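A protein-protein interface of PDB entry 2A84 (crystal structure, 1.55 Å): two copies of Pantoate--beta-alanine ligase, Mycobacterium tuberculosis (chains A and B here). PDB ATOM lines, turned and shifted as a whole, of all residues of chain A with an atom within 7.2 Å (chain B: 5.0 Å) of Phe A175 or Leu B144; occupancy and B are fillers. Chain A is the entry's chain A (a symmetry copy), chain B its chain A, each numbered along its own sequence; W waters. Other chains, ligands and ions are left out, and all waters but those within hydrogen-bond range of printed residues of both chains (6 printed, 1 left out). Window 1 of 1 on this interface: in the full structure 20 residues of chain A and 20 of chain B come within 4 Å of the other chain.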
ATOM      1  N   THR A 117      24.379 -34.334   7.024  1.00  0.00           N
ATOM      2  CA  THR A 117      25.416 -33.405   6.550  1.00  0.00           C
ATOM      3  C   THR A 117      25.407 -33.287   5.051  1.00  0.00           C
ATOM      4  O   THR A 117      24.721 -34.022   4.374  1.00  0.00           O
ATOM      5  CB  THR A 117      26.821 -33.832   7.010  1.00  0.00           C
ATOM      6  OG1 THR A 117      27.139 -35.087   6.455  1.00  0.00           O
ATOM      7  CG2 THR A 117      26.911 -33.923   8.515  1.00  0.00           C
ATOM      8  N   VAL A 118      26.145 -32.332   4.540  1.00  0.00           N
ATOM      9  CA  VAL A 118      26.321 -32.175   3.097  1.00  0.00           C
ATOM     10  C   VAL A 118      27.577 -32.881   2.680  1.00  0.00           C
ATOM     11  O   VAL A 118      28.636 -32.706   3.334  1.00  0.00           O
ATOM     12  CB  VAL A 118      26.427 -30.704   2.736  1.00  0.00           C
ATOM     13  CG1 VAL A 118      26.748 -30.549   1.275  1.00  0.00           C
ATOM     14  CG2 VAL A 118      25.188 -29.954   3.150  1.00  0.00           C
ATOM     15  N   GLN A 119      27.514 -33.670   1.589  1.00  0.00           N
ATOM     16  CA  GLN A 119      28.664 -34.312   0.993  1.00  0.00           C
ATOM     17  C   GLN A 119      28.985 -33.527  -0.274  1.00  0.00           C
ATOM     18  O   GLN A 119      28.243 -33.585  -1.239  1.00  0.00           O
ATOM     19  CB  GLN A 119      28.277 -35.711   0.593  1.00  0.00           C
ATOM     20  CG  GLN A 119      29.385 -36.430  -0.155  1.00  0.00           C
ATOM     21  CD  GLN A 119      29.931 -37.518   0.670  1.00  0.00           C
ATOM     22  OE1 GLN A 119      29.330 -38.599   0.752  1.00  0.00           O
ATOM     23  NE2 GLN A 119      31.034 -37.245   1.346  1.00  0.00           N
ATOM     24  N   LEU A 140      30.278 -26.492   3.763  1.00  0.00           N
ATOM     25  CA  LEU A 140      29.014 -26.518   3.002  1.00  0.00           C
ATOM     26  C   LEU A 140      27.847 -26.837   3.946  1.00  0.00           C
ATOM     27  O   LEU A 140      26.723 -26.357   3.715  1.00  0.00           O
ATOM     28  CB  LEU A 140      29.052 -27.494   1.853  1.00  0.00           C
ATOM     29  CG  LEU A 140      29.578 -26.839   0.563  1.00  0.00           C
ATOM     30  CD1 LEU A 140      30.880 -26.131   0.699  1.00  0.00           C
ATOM     31  CD2 LEU A 140      29.488 -27.891  -0.610  1.00  0.00           C
ATOM     32  N   LEU A 144      24.936 -24.129   4.313  1.00  0.00           N
ATOM     33  CA  LEU A 144      23.568 -24.506   4.005  1.00  0.00           C
ATOM     34  C   LEU A 144      22.636 -24.159   5.193  1.00  0.00           C
ATOM     35  O   LEU A 144      21.557 -23.569   5.048  1.00  0.00           O
ATOM     36  CB  LEU A 144      23.427 -25.990   3.653  1.00  0.00           C
ATOM     37  CG  LEU A 144      22.015 -26.506   3.420  1.00  0.00           C
ATOM     38  CD1 LEU A 144      21.443 -25.823   2.187  1.00  0.00           C
ATOM     39  CD2 LEU A 144      21.998 -27.991   3.220  1.00  0.00           C
ATOM     40  N   GLN A 148      19.502 -21.451   5.354  1.00  0.00           N
ATOM     41  CA  GLN A 148      18.142 -21.789   5.680  1.00  0.00           C
ATOM     42  C   GLN A 148      17.565 -21.009   6.861  1.00  0.00           C
ATOM     43  O   GLN A 148      16.357 -20.703   6.922  1.00  0.00           O
ATOM     44  CB  GLN A 148      18.056 -23.299   5.964  1.00  0.00           C
ATOM     45  CG  GLN A 148      18.418 -24.149   4.740  1.00  0.00           C
ATOM     46  CD  GLN A 148      17.584 -23.873   3.497  1.00  0.00           C
ATOM     47  OE1 GLN A 148      18.122 -23.834   2.380  1.00  0.00           O
ATOM     48  NE2 GLN A 148      16.339 -23.774   3.651  1.00  0.00           N
ATOM     49  N   ARG A 169      29.074 -22.104  -4.938  1.00  0.00           N
ATOM     50  CA  ARG A 169      28.248 -22.042  -6.157  1.00  0.00           C
ATOM     51  C   ARG A 169      27.723 -23.435  -6.519  1.00  0.00           C
ATOM     52  O   ARG A 169      26.553 -23.581  -6.968  1.00  0.00           O
ATOM     53  CB  ARG A 169      29.039 -21.438  -7.294  1.00  0.00           C
ATOM     54  CG  ARG A 169      29.405 -19.974  -7.065  1.00  0.00           C
ATOM     55  CD  ARG A 169      29.835 -19.306  -8.354  1.00  0.00           C
ATOM     56  NE  ARG A 169      30.439 -17.989  -8.164  1.00  0.00           N
ATOM     57  CZ  ARG A 169      29.794 -16.871  -7.892  1.00  0.00           C
ATOM     58  NH1 ARG A 169      28.483 -16.799  -7.827  1.00  0.00           N
ATOM     59  NH2 ARG A 169      30.503 -15.759  -7.757  1.00  0.00           N
ATOM     60  N   GLN A 170      28.550 -24.470  -6.344  1.00  0.00           N
ATOM     61  CA  GLN A 170      28.069 -25.852  -6.612  1.00  0.00           C
ATOM     62  C   GLN A 170      26.919 -26.228  -5.668  1.00  0.00           C
ATOM     63  O   GLN A 170      25.905 -26.814  -6.090  1.00  0.00           O
ATOM     64  CB  GLN A 170      29.209 -26.866  -6.503  1.00  0.00           C
ATOM     65  CG  GLN A 170      30.293 -26.669  -7.548  1.00  0.00           C
ATOM     66  CD  GLN A 170      31.317 -27.794  -7.596  1.00  0.00           C
ATOM     67  OE1 GLN A 170      31.285 -28.746  -6.772  1.00  0.00           O
ATOM     68  NE2 GLN A 170      32.226 -27.719  -8.600  1.00  0.00           N
ATOM     69  N   LEU A 171      27.067 -25.931  -4.378  1.00  0.00           N
ATOM     70  CA  LEU A 171      26.013 -26.187  -3.390  1.00  0.00           C
ATOM     71  C   LEU A 171      24.725 -25.522  -3.851  1.00  0.00           C
ATOM     72  O   LEU A 171      23.657 -26.097  -3.865  1.00  0.00           O
ATOM     73  CB  LEU A 171      26.441 -25.580  -2.051  1.00  0.00           C
ATOM     74  CG  LEU A 171      25.408 -25.609  -0.922  1.00  0.00           C
ATOM     75  CD1 LEU A 171      25.283 -26.969  -0.231  1.00  0.00           C
ATOM     76  CD2 LEU A 171      25.803 -24.593   0.187  1.00  0.00           C
ATOM     77  N   VAL A 172      24.809 -24.243  -4.214  1.00  0.00           N
ATOM     78  CA  VAL A 172      23.592 -23.469  -4.562  1.00  0.00           C
ATOM     79  C   VAL A 172      22.942 -24.053  -5.825  1.00  0.00           C
ATOM     80  O   VAL A 172      21.722 -24.194  -5.899  1.00  0.00           O
ATOM     81  CB  VAL A 172      23.982 -21.983  -4.641  1.00  0.00           C
ATOM     82  CG1 VAL A 172      22.941 -21.166  -5.369  1.00  0.00           C
ATOM     83  CG2 VAL A 172      24.266 -21.477  -3.245  1.00  0.00           C
ATOM     84  N   ALA A 173      23.759 -24.371  -6.833  1.00  0.00           N
ATOM     85  CA  ALA A 173      23.211 -24.935  -8.072  1.00  0.00           C
ATOM     86  C   ALA A 173      22.617 -26.297  -7.790  1.00  0.00           C
ATOM     87  O   ALA A 173      21.493 -26.620  -8.214  1.00  0.00           O
ATOM     88  CB  ALA A 173      24.282 -25.046  -9.103  1.00  0.00           C
ATOM     89  N   ASP A 174      23.392 -27.149  -7.119  1.00  0.00           N
ATOM     90  CA  ASP A 174      23.017 -28.547  -6.966  1.00  0.00           C
ATOM     91  C   ASP A 174      21.804 -28.786  -6.103  1.00  0.00           C
ATOM     92  O   ASP A 174      21.087 -29.781  -6.280  1.00  0.00           O
ATOM     93  CB  ASP A 174      24.181 -29.310  -6.379  1.00  0.00           C
ATOM     94  CG  ASP A 174      25.372 -29.425  -7.334  1.00  0.00           C
ATOM     95  OD1 ASP A 174      25.242 -29.075  -8.553  1.00  0.00           O
ATOM     96  OD2 ASP A 174      26.499 -29.889  -6.931  1.00  0.00           O
ATOM     97  N   PHE A 175      21.587 -27.921  -5.119  1.00  0.00           N
ATOM     98  CA  PHE A 175      20.427 -28.018  -4.240  1.00  0.00           C
ATOM     99  C   PHE A 175      19.333 -26.986  -4.574  1.00  0.00           C
ATOM    100  O   PHE A 175      18.362 -26.835  -3.814  1.00  0.00           O
ATOM    101  CB  PHE A 175      20.876 -27.834  -2.767  1.00  0.00           C
ATOM    102  CG  PHE A 175      21.684 -28.995  -2.194  1.00  0.00           C
ATOM    103  CD1 PHE A 175      22.331 -28.838  -0.970  1.00  0.00           C
ATOM    104  CD2 PHE A 175      21.728 -30.220  -2.791  1.00  0.00           C
ATOM    105  CE1 PHE A 175      23.038 -29.881  -0.416  1.00  0.00           C
ATOM    106  CE2 PHE A 175      22.460 -31.263  -2.219  1.00  0.00           C
ATOM    107  CZ  PHE A 175      23.081 -31.062  -1.023  1.00  0.00           C
ATOM    108  N   ASN A 176      19.486 -26.301  -5.709  1.00  0.00           N
ATOM    109  CA  ASN A 176      18.428 -25.415  -6.223  1.00  0.00           C
ATOM    110  C   ASN A 176      18.133 -24.294  -5.244  1.00  0.00           C
ATOM    111  O   ASN A 176      16.988 -23.847  -5.088  1.00  0.00           O
ATOM    112  CB  ASN A 176      17.155 -26.189  -6.543  1.00  0.00           C
ATOM    113  CG  ASN A 176      17.399 -27.322  -7.519  1.00  0.00           C
ATOM    114  OD1 ASN A 176      17.626 -28.446  -7.109  1.00  0.00           O
ATOM    115  ND2 ASN A 176      17.391 -27.015  -8.827  1.00  0.00           N
ATOM    116  N   LEU A 177      19.179 -23.798  -4.616  1.00  0.00           N
ATOM    117  CA  LEU A 177      18.987 -22.746  -3.584  1.00  0.00           C
ATOM    118  C   LEU A 177      18.675 -21.400  -4.240  1.00  0.00           C
ATOM    119  O   LEU A 177      19.340 -21.018  -5.183  1.00  0.00           O
ATOM    120  CB  LEU A 177      20.164 -22.631  -2.618  1.00  0.00           C
ATOM    121  CG  LEU A 177      20.607 -23.946  -1.953  1.00  0.00           C
ATOM    122  CD1 LEU A 177      21.815 -23.760  -1.011  1.00  0.00           C
ATOM    123  CD2 LEU A 177      19.571 -24.545  -1.272  1.00  0.00           C
ATOM    124  N   ASP A 178      17.683 -20.701  -3.688  1.00  0.00           N
ATOM    125  CA  ASP A 178      17.211 -19.461  -4.229  1.00  0.00           C
ATOM    126  C   ASP A 178      17.952 -18.367  -3.513  1.00  0.00           C
ATOM    127  O   ASP A 178      17.380 -17.700  -2.648  1.00  0.00           O
ATOM    128  CB  ASP A 178      15.734 -19.312  -3.873  1.00  0.00           C
ATOM    129  CG  ASP A 178      15.097 -18.140  -4.491  1.00  0.00           C
ATOM    130  OD1 ASP A 178      15.668 -17.557  -5.451  1.00  0.00           O
ATOM    131  OD2 ASP A 178      13.980 -17.753  -4.071  1.00  0.00           O
ATOM    132  N   THR B 116      27.069 -32.428  -5.512  1.00  0.00           N
ATOM    133  CA  THR B 116      26.788 -32.244  -4.086  1.00  0.00           C
ATOM    134  C   THR B 116      25.569 -33.076  -3.716  1.00  0.00           C
ATOM    135  O   THR B 116      24.551 -33.026  -4.408  1.00  0.00           O
ATOM    136  CB  THR B 116      26.436 -30.758  -3.790  1.00  0.00           C
ATOM    137  OG1 THR B 116      27.366 -29.870  -4.439  1.00  0.00           O
ATOM    138  CG2 THR B 116      26.490 -30.476  -2.279  1.00  0.00           C
ATOM    139  N   THR B 117      25.636 -33.781  -2.584  1.00  0.00           N
ATOM    140  CA  THR B 117      24.528 -34.627  -2.114  1.00  0.00           C
ATOM    141  C   THR B 117      24.334 -34.505  -0.628  1.00  0.00           C
ATOM    142  O   THR B 117      25.133 -33.904   0.056  1.00  0.00           O
ATOM    143  CB  THR B 117      24.745 -36.107  -2.472  1.00  0.00           C
ATOM    144  OG1 THR B 117      25.900 -36.585  -1.823  1.00  0.00           O
ATOM    145  CG2 THR B 117      24.900 -36.304  -3.961  1.00  0.00           C
ATOM    146  N   VAL B 118      23.245 -35.048  -0.139  1.00  0.00           N
ATOM    147  CA  VAL B 118      22.986 -35.107   1.299  1.00  0.00           C
ATOM    148  C   VAL B 118      23.456 -36.431   1.825  1.00  0.00           C
ATOM    149  O   VAL B 118      23.146 -37.488   1.218  1.00  0.00           O
ATOM    150  CB  VAL B 118      21.500 -34.956   1.572  1.00  0.00           C
ATOM    151  CG1 VAL B 118      21.218 -35.156   3.036  1.00  0.00           C
ATOM    152  CG2 VAL B 118      20.984 -33.641   1.047  1.00  0.00           C
ATOM    153  N   VAL B 139      16.936 -40.252  -1.452  1.00  0.00           N
ATOM    154  CA  VAL B 139      15.665 -39.663  -1.043  1.00  0.00           C
ATOM    155  C   VAL B 139      15.843 -38.264  -0.449  1.00  0.00           C
ATOM    156  O   VAL B 139      15.154 -37.269  -0.848  1.00  0.00           O
ATOM    157  CB  VAL B 139      14.977 -40.536   0.002  1.00  0.00           C
ATOM    158  CG1 VAL B 139      13.794 -39.824   0.603  1.00  0.00           C
ATOM    159  CG2 VAL B 139      14.577 -41.821  -0.598  1.00  0.00           C
ATOM    160  N   LEU B 140      16.780 -38.146   0.490  1.00  0.00           N
ATOM    161  CA  LEU B 140      16.970 -36.857   1.184  1.00  0.00           C
ATOM    162  C   LEU B 140      17.524 -35.816   0.201  1.00  0.00           C
ATOM    163  O   LEU B 140      17.221 -34.618   0.342  1.00  0.00           O
ATOM    164  CB  LEU B 140      17.865 -36.978   2.391  1.00  0.00           C
ATOM    165  CG  LEU B 140      17.066 -37.311   3.664  1.00  0.00           C
ATOM    166  CD1 LEU B 140      16.164 -38.490   3.554  1.00  0.00           C
ATOM    167  CD2 LEU B 140      18.055 -37.317   4.894  1.00  0.00           C
ATOM    168  N   THR B 141      18.396 -36.233  -0.728  1.00  0.00           N
ATOM    169  CA  THR B 141      18.898 -35.294  -1.752  1.00  0.00           C
ATOM    170  C   THR B 141      17.739 -34.743  -2.603  1.00  0.00           C
ATOM    171  O   THR B 141      17.635 -33.513  -2.828  1.00  0.00           O
ATOM    172  CB  THR B 141      19.968 -35.950  -2.580  1.00  0.00           C
ATOM    173  OG1 THR B 141      21.076 -36.347  -1.721  1.00  0.00           O
ATOM    174  CG2 THR B 141      20.503 -34.965  -3.636  1.00  0.00           C
ATOM    175  N   VAL B 142      16.920 -35.667  -3.110  1.00  0.00           N
ATOM    176  CA  VAL B 142      15.803 -35.243  -3.958  1.00  0.00           C
ATOM    177  C   VAL B 142      14.823 -34.401  -3.178  1.00  0.00           C
ATOM    178  O   VAL B 142      14.399 -33.358  -3.644  1.00  0.00           O
ATOM    179  CB  VAL B 142      15.094 -36.437  -4.549  1.00  0.00           C
ATOM    180  CG1 VAL B 142      13.756 -35.962  -5.228  1.00  0.00           C
ATOM    181  CG2 VAL B 142      15.956 -37.124  -5.482  1.00  0.00           C
ATOM    182  N   VAL B 143      14.477 -34.791  -1.950  1.00  0.00           N
ATOM    183  CA  VAL B 143      13.495 -34.013  -1.153  1.00  0.00           C
ATOM    184  C   VAL B 143      14.048 -32.609  -0.862  1.00  0.00           C
ATOM    185  O   VAL B 143      13.345 -31.581  -0.932  1.00  0.00           O
ATOM    186  CB  VAL B 143      13.102 -34.738   0.111  1.00  0.00           C
ATOM    187  CG1 VAL B 143      12.327 -33.871   1.063  1.00  0.00           C
ATOM    188  CG2 VAL B 143      12.285 -35.998  -0.239  1.00  0.00           C
ATOM    189  N   LEU B 144      15.347 -32.541  -0.488  1.00  0.00           N
ATOM    190  CA  LEU B 144      15.924 -31.234  -0.230  1.00  0.00           C
ATOM    191  C   LEU B 144      15.796 -30.335  -1.485  1.00  0.00           C
ATOM    192  O   LEU B 144      15.382 -29.168  -1.434  1.00  0.00           O
ATOM    193  CB  LEU B 144      17.391 -31.309   0.206  1.00  0.00           C
ATOM    194  CG  LEU B 144      18.116 -29.984   0.395  1.00  0.00           C
ATOM    195  CD1 LEU B 144      17.470 -29.235   1.552  1.00  0.00           C
ATOM    196  CD2 LEU B 144      19.571 -30.191   0.687  1.00  0.00           C
ATOM    197  N   LYS B 145      16.152 -30.890  -2.646  1.00  0.00           N
ATOM    198  CA  LYS B 145      16.020 -30.119  -3.924  1.00  0.00           C
ATOM    199  C   LYS B 145      14.573 -29.684  -4.146  1.00  0.00           C
ATOM    200  O   LYS B 145      14.309 -28.525  -4.446  1.00  0.00           O
ATOM    201  CB  LYS B 145      16.524 -30.929  -5.107  1.00  0.00           C
ATOM    202  CG  LYS B 145      18.053 -31.113  -5.044  1.00  0.00           C
ATOM    203  CD  LYS B 145      18.620 -32.194  -5.984  1.00  0.00           C
ATOM    204  CE  LYS B 145      18.274 -31.934  -7.461  1.00  0.00           C
ATOM    205  NZ  LYS B 145      18.942 -30.683  -7.974  1.00  0.00           N
ATOM    206  N   LEU B 146      13.634 -30.610  -3.974  1.00  0.00           N
ATOM    207  CA  LEU B 146      12.204 -30.261  -4.198  1.00  0.00           C
ATOM    208  C   LEU B 146      11.780 -29.151  -3.252  1.00  0.00           C
ATOM    209  O   LEU B 146      11.077 -28.235  -3.633  1.00  0.00           O
ATOM    210  CB  LEU B 146      11.330 -31.478  -4.020  1.00  0.00           C
ATOM    211  CG  LEU B 146      11.526 -32.562  -5.075  1.00  0.00           C
ATOM    212  CD1 LEU B 146      10.739 -33.828  -4.716  1.00  0.00           C
ATOM    213  CD2 LEU B 146      11.117 -32.076  -6.471  1.00  0.00           C
ATOM    214  N   LEU B 147      12.210 -29.238  -1.982  1.00  0.00           N
ATOM    215  CA  LEU B 147      11.878 -28.206  -1.027  1.00  0.00           C
ATOM    216  C   LEU B 147      12.424 -26.838  -1.424  1.00  0.00           C
ATOM    217  O   LEU B 147      11.825 -25.804  -1.186  1.00  0.00           O
ATOM    218  CB  LEU B 147      12.352 -28.547   0.402  1.00  0.00           C
ATOM    219  CG  LEU B 147      11.615 -29.720   1.067  1.00  0.00           C
ATOM    220  CD1 LEU B 147      12.353 -30.192   2.343  1.00  0.00           C
ATOM    221  CD2 LEU B 147      10.210 -29.271   1.400  1.00  0.00           C
ATOM    222  N   GLN B 148      13.645 -26.826  -1.980  1.00  0.00           N
ATOM    223  CA  GLN B 148      14.215 -25.560  -2.356  1.00  0.00           C
ATOM    224  C   GLN B 148      13.603 -24.941  -3.612  1.00  0.00           C
ATOM    225  O   GLN B 148      13.500 -23.706  -3.756  1.00  0.00           O
ATOM    226  CB  GLN B 148      15.732 -25.732  -2.550  1.00  0.00           C
ATOM    227  CG  GLN B 148      16.447 -26.148  -1.257  1.00  0.00           C
ATOM    228  CD  GLN B 148      16.244 -25.205  -0.081  1.00  0.00           C
ATOM    229  OE1 GLN B 148      16.059 -25.660   1.059  1.00  0.00           O
ATOM    230  NE2 GLN B 148      16.357 -23.972  -0.305  1.00  0.00           N
ATOM    231  N   LEU B 171      16.317 -34.385   8.400  1.00  0.00           N
ATOM    232  CA  LEU B 171      16.792 -33.449   7.374  1.00  0.00           C
ATOM    233  C   LEU B 171      16.321 -32.045   7.724  1.00  0.00           C
ATOM    234  O   LEU B 171      17.061 -31.083   7.718  1.00  0.00           O
ATOM    235  CB  LEU B 171      16.196 -33.858   6.025  1.00  0.00           C
ATOM    236  CG  LEU B 171      16.452 -32.915   4.847  1.00  0.00           C
ATOM    237  CD1 LEU B 171      17.849 -33.050   4.236  1.00  0.00           C
ATOM    238  CD2 LEU B 171      15.445 -33.211   3.699  1.00  0.00           C
ATOM    239  N   PHE B 175      19.127 -29.255   8.971  1.00  0.00           N
ATOM    240  CA  PHE B 175      19.457 -28.183   8.040  1.00  0.00           C
ATOM    241  C   PHE B 175      18.599 -26.920   8.250  1.00  0.00           C
ATOM    242  O   PHE B 175      18.649 -25.986   7.433  1.00  0.00           O
ATOM    243  CB  PHE B 175      19.281 -28.687   6.584  1.00  0.00           C
ATOM    244  CG  PHE B 175      20.324 -29.703   6.128  1.00  0.00           C
ATOM    245  CD1 PHE B 175      20.129 -30.393   4.933  1.00  0.00           C
ATOM    246  CD2 PHE B 175      21.492 -29.905   6.802  1.00  0.00           C
ATOM    247  CE1 PHE B 175      21.072 -31.289   4.483  1.00  0.00           C
ATOM    248  CE2 PHE B 175      22.432 -30.827   6.336  1.00  0.00           C
ATOM    249  CZ  PHE B 175      22.197 -31.482   5.164  1.00  0.00           C
ATOM    250  N   LEU B 177      15.481 -26.259   8.086  1.00  0.00           N
ATOM    251  CA  LEU B 177      14.530 -25.967   6.981  1.00  0.00           C
ATOM    252  C   LEU B 177      13.221 -25.405   7.535  1.00  0.00           C
ATOM    253  O   LEU B 177      12.686 -25.941   8.486  1.00  0.00           O
ATOM    254  CB  LEU B 177      14.277 -27.169   6.074  1.00  0.00           C
ATOM    255  CG  LEU B 177      15.537 -27.856   5.516  1.00  0.00           C
ATOM    256  CD1 LEU B 177      15.208 -29.075   4.630  1.00  0.00           C
ATOM    257  CD2 LEU B 177      16.331 -26.972   4.820  1.00  0.00           C
HETATM  258  O   HOH W   1      18.379 -28.900 -10.893  1.00  0.00           O
HETATM  259  O   HOH W   2      15.058 -22.505  -6.329  1.00  0.00           O
HETATM  260  O   HOH W   3      15.643 -22.141  -2.245  1.00  0.00           O
HETATM  261  O   HOH W   4      20.778 -28.886  -9.825  1.00  0.00           O
HETATM  262  O   HOH W   5      30.174 -29.719  -4.345  1.00  0.00           O
HETATM  263  O   HOH W   6      21.882 -31.937  -8.288  1.00  0.00           O
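The side-chain amide oxygen of Gln B148 lies close to the side-chain amide oxygen of Gln A148 (3.1 Å).
O of Thr B117 lies within hydrogen-bond range of N of Gln A119 (2.8 Å).
NZ of Lys B145 lies within hydrogen-bond range of O of Asp A174 (2.9 Å).
The side-chain hydroxyl (OG1) of Thr B116 lies within hydrogen-bond range of the side-chain carboxylate (OD2) of Asp A174 (2.6 Å).
The side-chain amide oxygen (OD1) of Asn A176 is in hydrogen-bond range of the side-chain amino group (NZ) of Lys B145 (2.7 Å).
OG1 of Thr B141 lies within hydrogen-bond range of N of Val B118 (3.0 Å).
The backbone carbonyl oxygen of Val A172 is in hydrogen-bond range of the backbone NH of Leu A177.
Among the printed residues, pairs that only touch across the chains: Thr A117 with Val B118 (3.7 Å), Thr A117 with Phe B175 (3.7 Å), Val A118 with Thr B116 (3.6 Å), Val A118 with Thr B117 (3.7 Å), Val A118 with Phe B175 (3.9 Å), Gln A119 with Thr B116 (3.5 Å), Leu A144 with Phe B175 (3.5 Å), Gln A148 with Phe B175 (3.1 Å), Gln A148 with Leu B177 (3.4 Å), Gln A170 with Thr B116 (3.8 Å), Leu A171 with Thr B116 (3.95 Å), Phe A175 with Thr B116 (3.5 Å), Phe A175 with Thr B117 (3.7 Å), Phe A175 with Val B118 (3.9 Å), Phe A175 with Leu B144 (3.5 Å), Phe A175 with Lys B145 (3.98 Å), Phe A175 with Gln B148 (3.1 Å), Asn A176 with Gln B148 (3.4 Å) and Leu A177 with Gln B148 (3.4 Å).
Of the printed residues of chain B, Phe A175 touches Thr B116 (3.5 Å), Thr B117 (3.7 Å), Val B118 (3.9 Å), Leu B144 (3.5 Å), Lys B145 (3.98 Å) and Gln B148 (3.1 Å).
Of chain A, only Phe A175 comes within 4 Å of Leu B144.
Printed residues of chain B within 4 Å of Leu A144: Phe B175.
Of the printed residues of chain A, Gln B148 touches Gln A148 (3.1 Å), Phe A175 (3.1 Å), Asn A176 (3.4 Å) and Leu A177 (3.4 Å).
Leu B171 touches none of the printed residues of chain A.
The nearest printed residue of chain B that does not touch Phe A175 is Thr B141 (4.4 Å).
The nearest printed residue of chain B that does not touch Gln A170 is Thr B117 (7.8 Å).
Of the 16 printed residues of chain A, 11 touch a printed residue of chain B.
Hydrophobic or aromatic side chains of chain A within 4 Å of the printed part of chain B: Val A118, Leu A144, Phe A175 and Leu A177.
Among the printed residues, no Asp or Glu carboxylate lies within 4 Å of a Lys or Arg side-chain nitrogen of the other chain.
Thr A117 touches Val B118, and with the chains exchanged Val A118 touches Thr B117.
Thr A117 touches Phe B175, and with the chains exchanged Phe A175 touches Thr B117.
Gln A148 touches its own counterpart, Gln B148.
Gln A148 touches Phe B175, and with the chains exchanged Phe A175 touches Gln B148.
Of the 24 pairs that touch across the chains among the printed residues, 13 have their exchanged pair printed and touching as well.
Water W2 lies within hydrogen-bond range of the backbone carbonyl oxygen (O) of Asn A176 and the backbone carbonyl oxygen (O) of Gln B148.
Water W3 lies within hydrogen-bond range of the side-chain amide nitrogen (NE2) of Gln B148 and the backbone NH (N) of Asp A178.
Water W5 lies within hydrogen-bond range of OG1 of Thr B116 (2.8 Å) and OE1 of Gln A170 (2.8 Å).
Water W4 bridges the backbone carbonyl oxygen (O) of Ala A173 and the side-chain amino group (NZ) of Lys B145.
Water W1 lies within hydrogen-bond range of ND2 of Asn A176 (3.0 Å) and NZ of Lys B145 (3.5 Å).
Water W6 bridges the backbone carbonyl oxygen (O) of Asp A174 and the side-chain amino group (NZ) of Lys B145.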
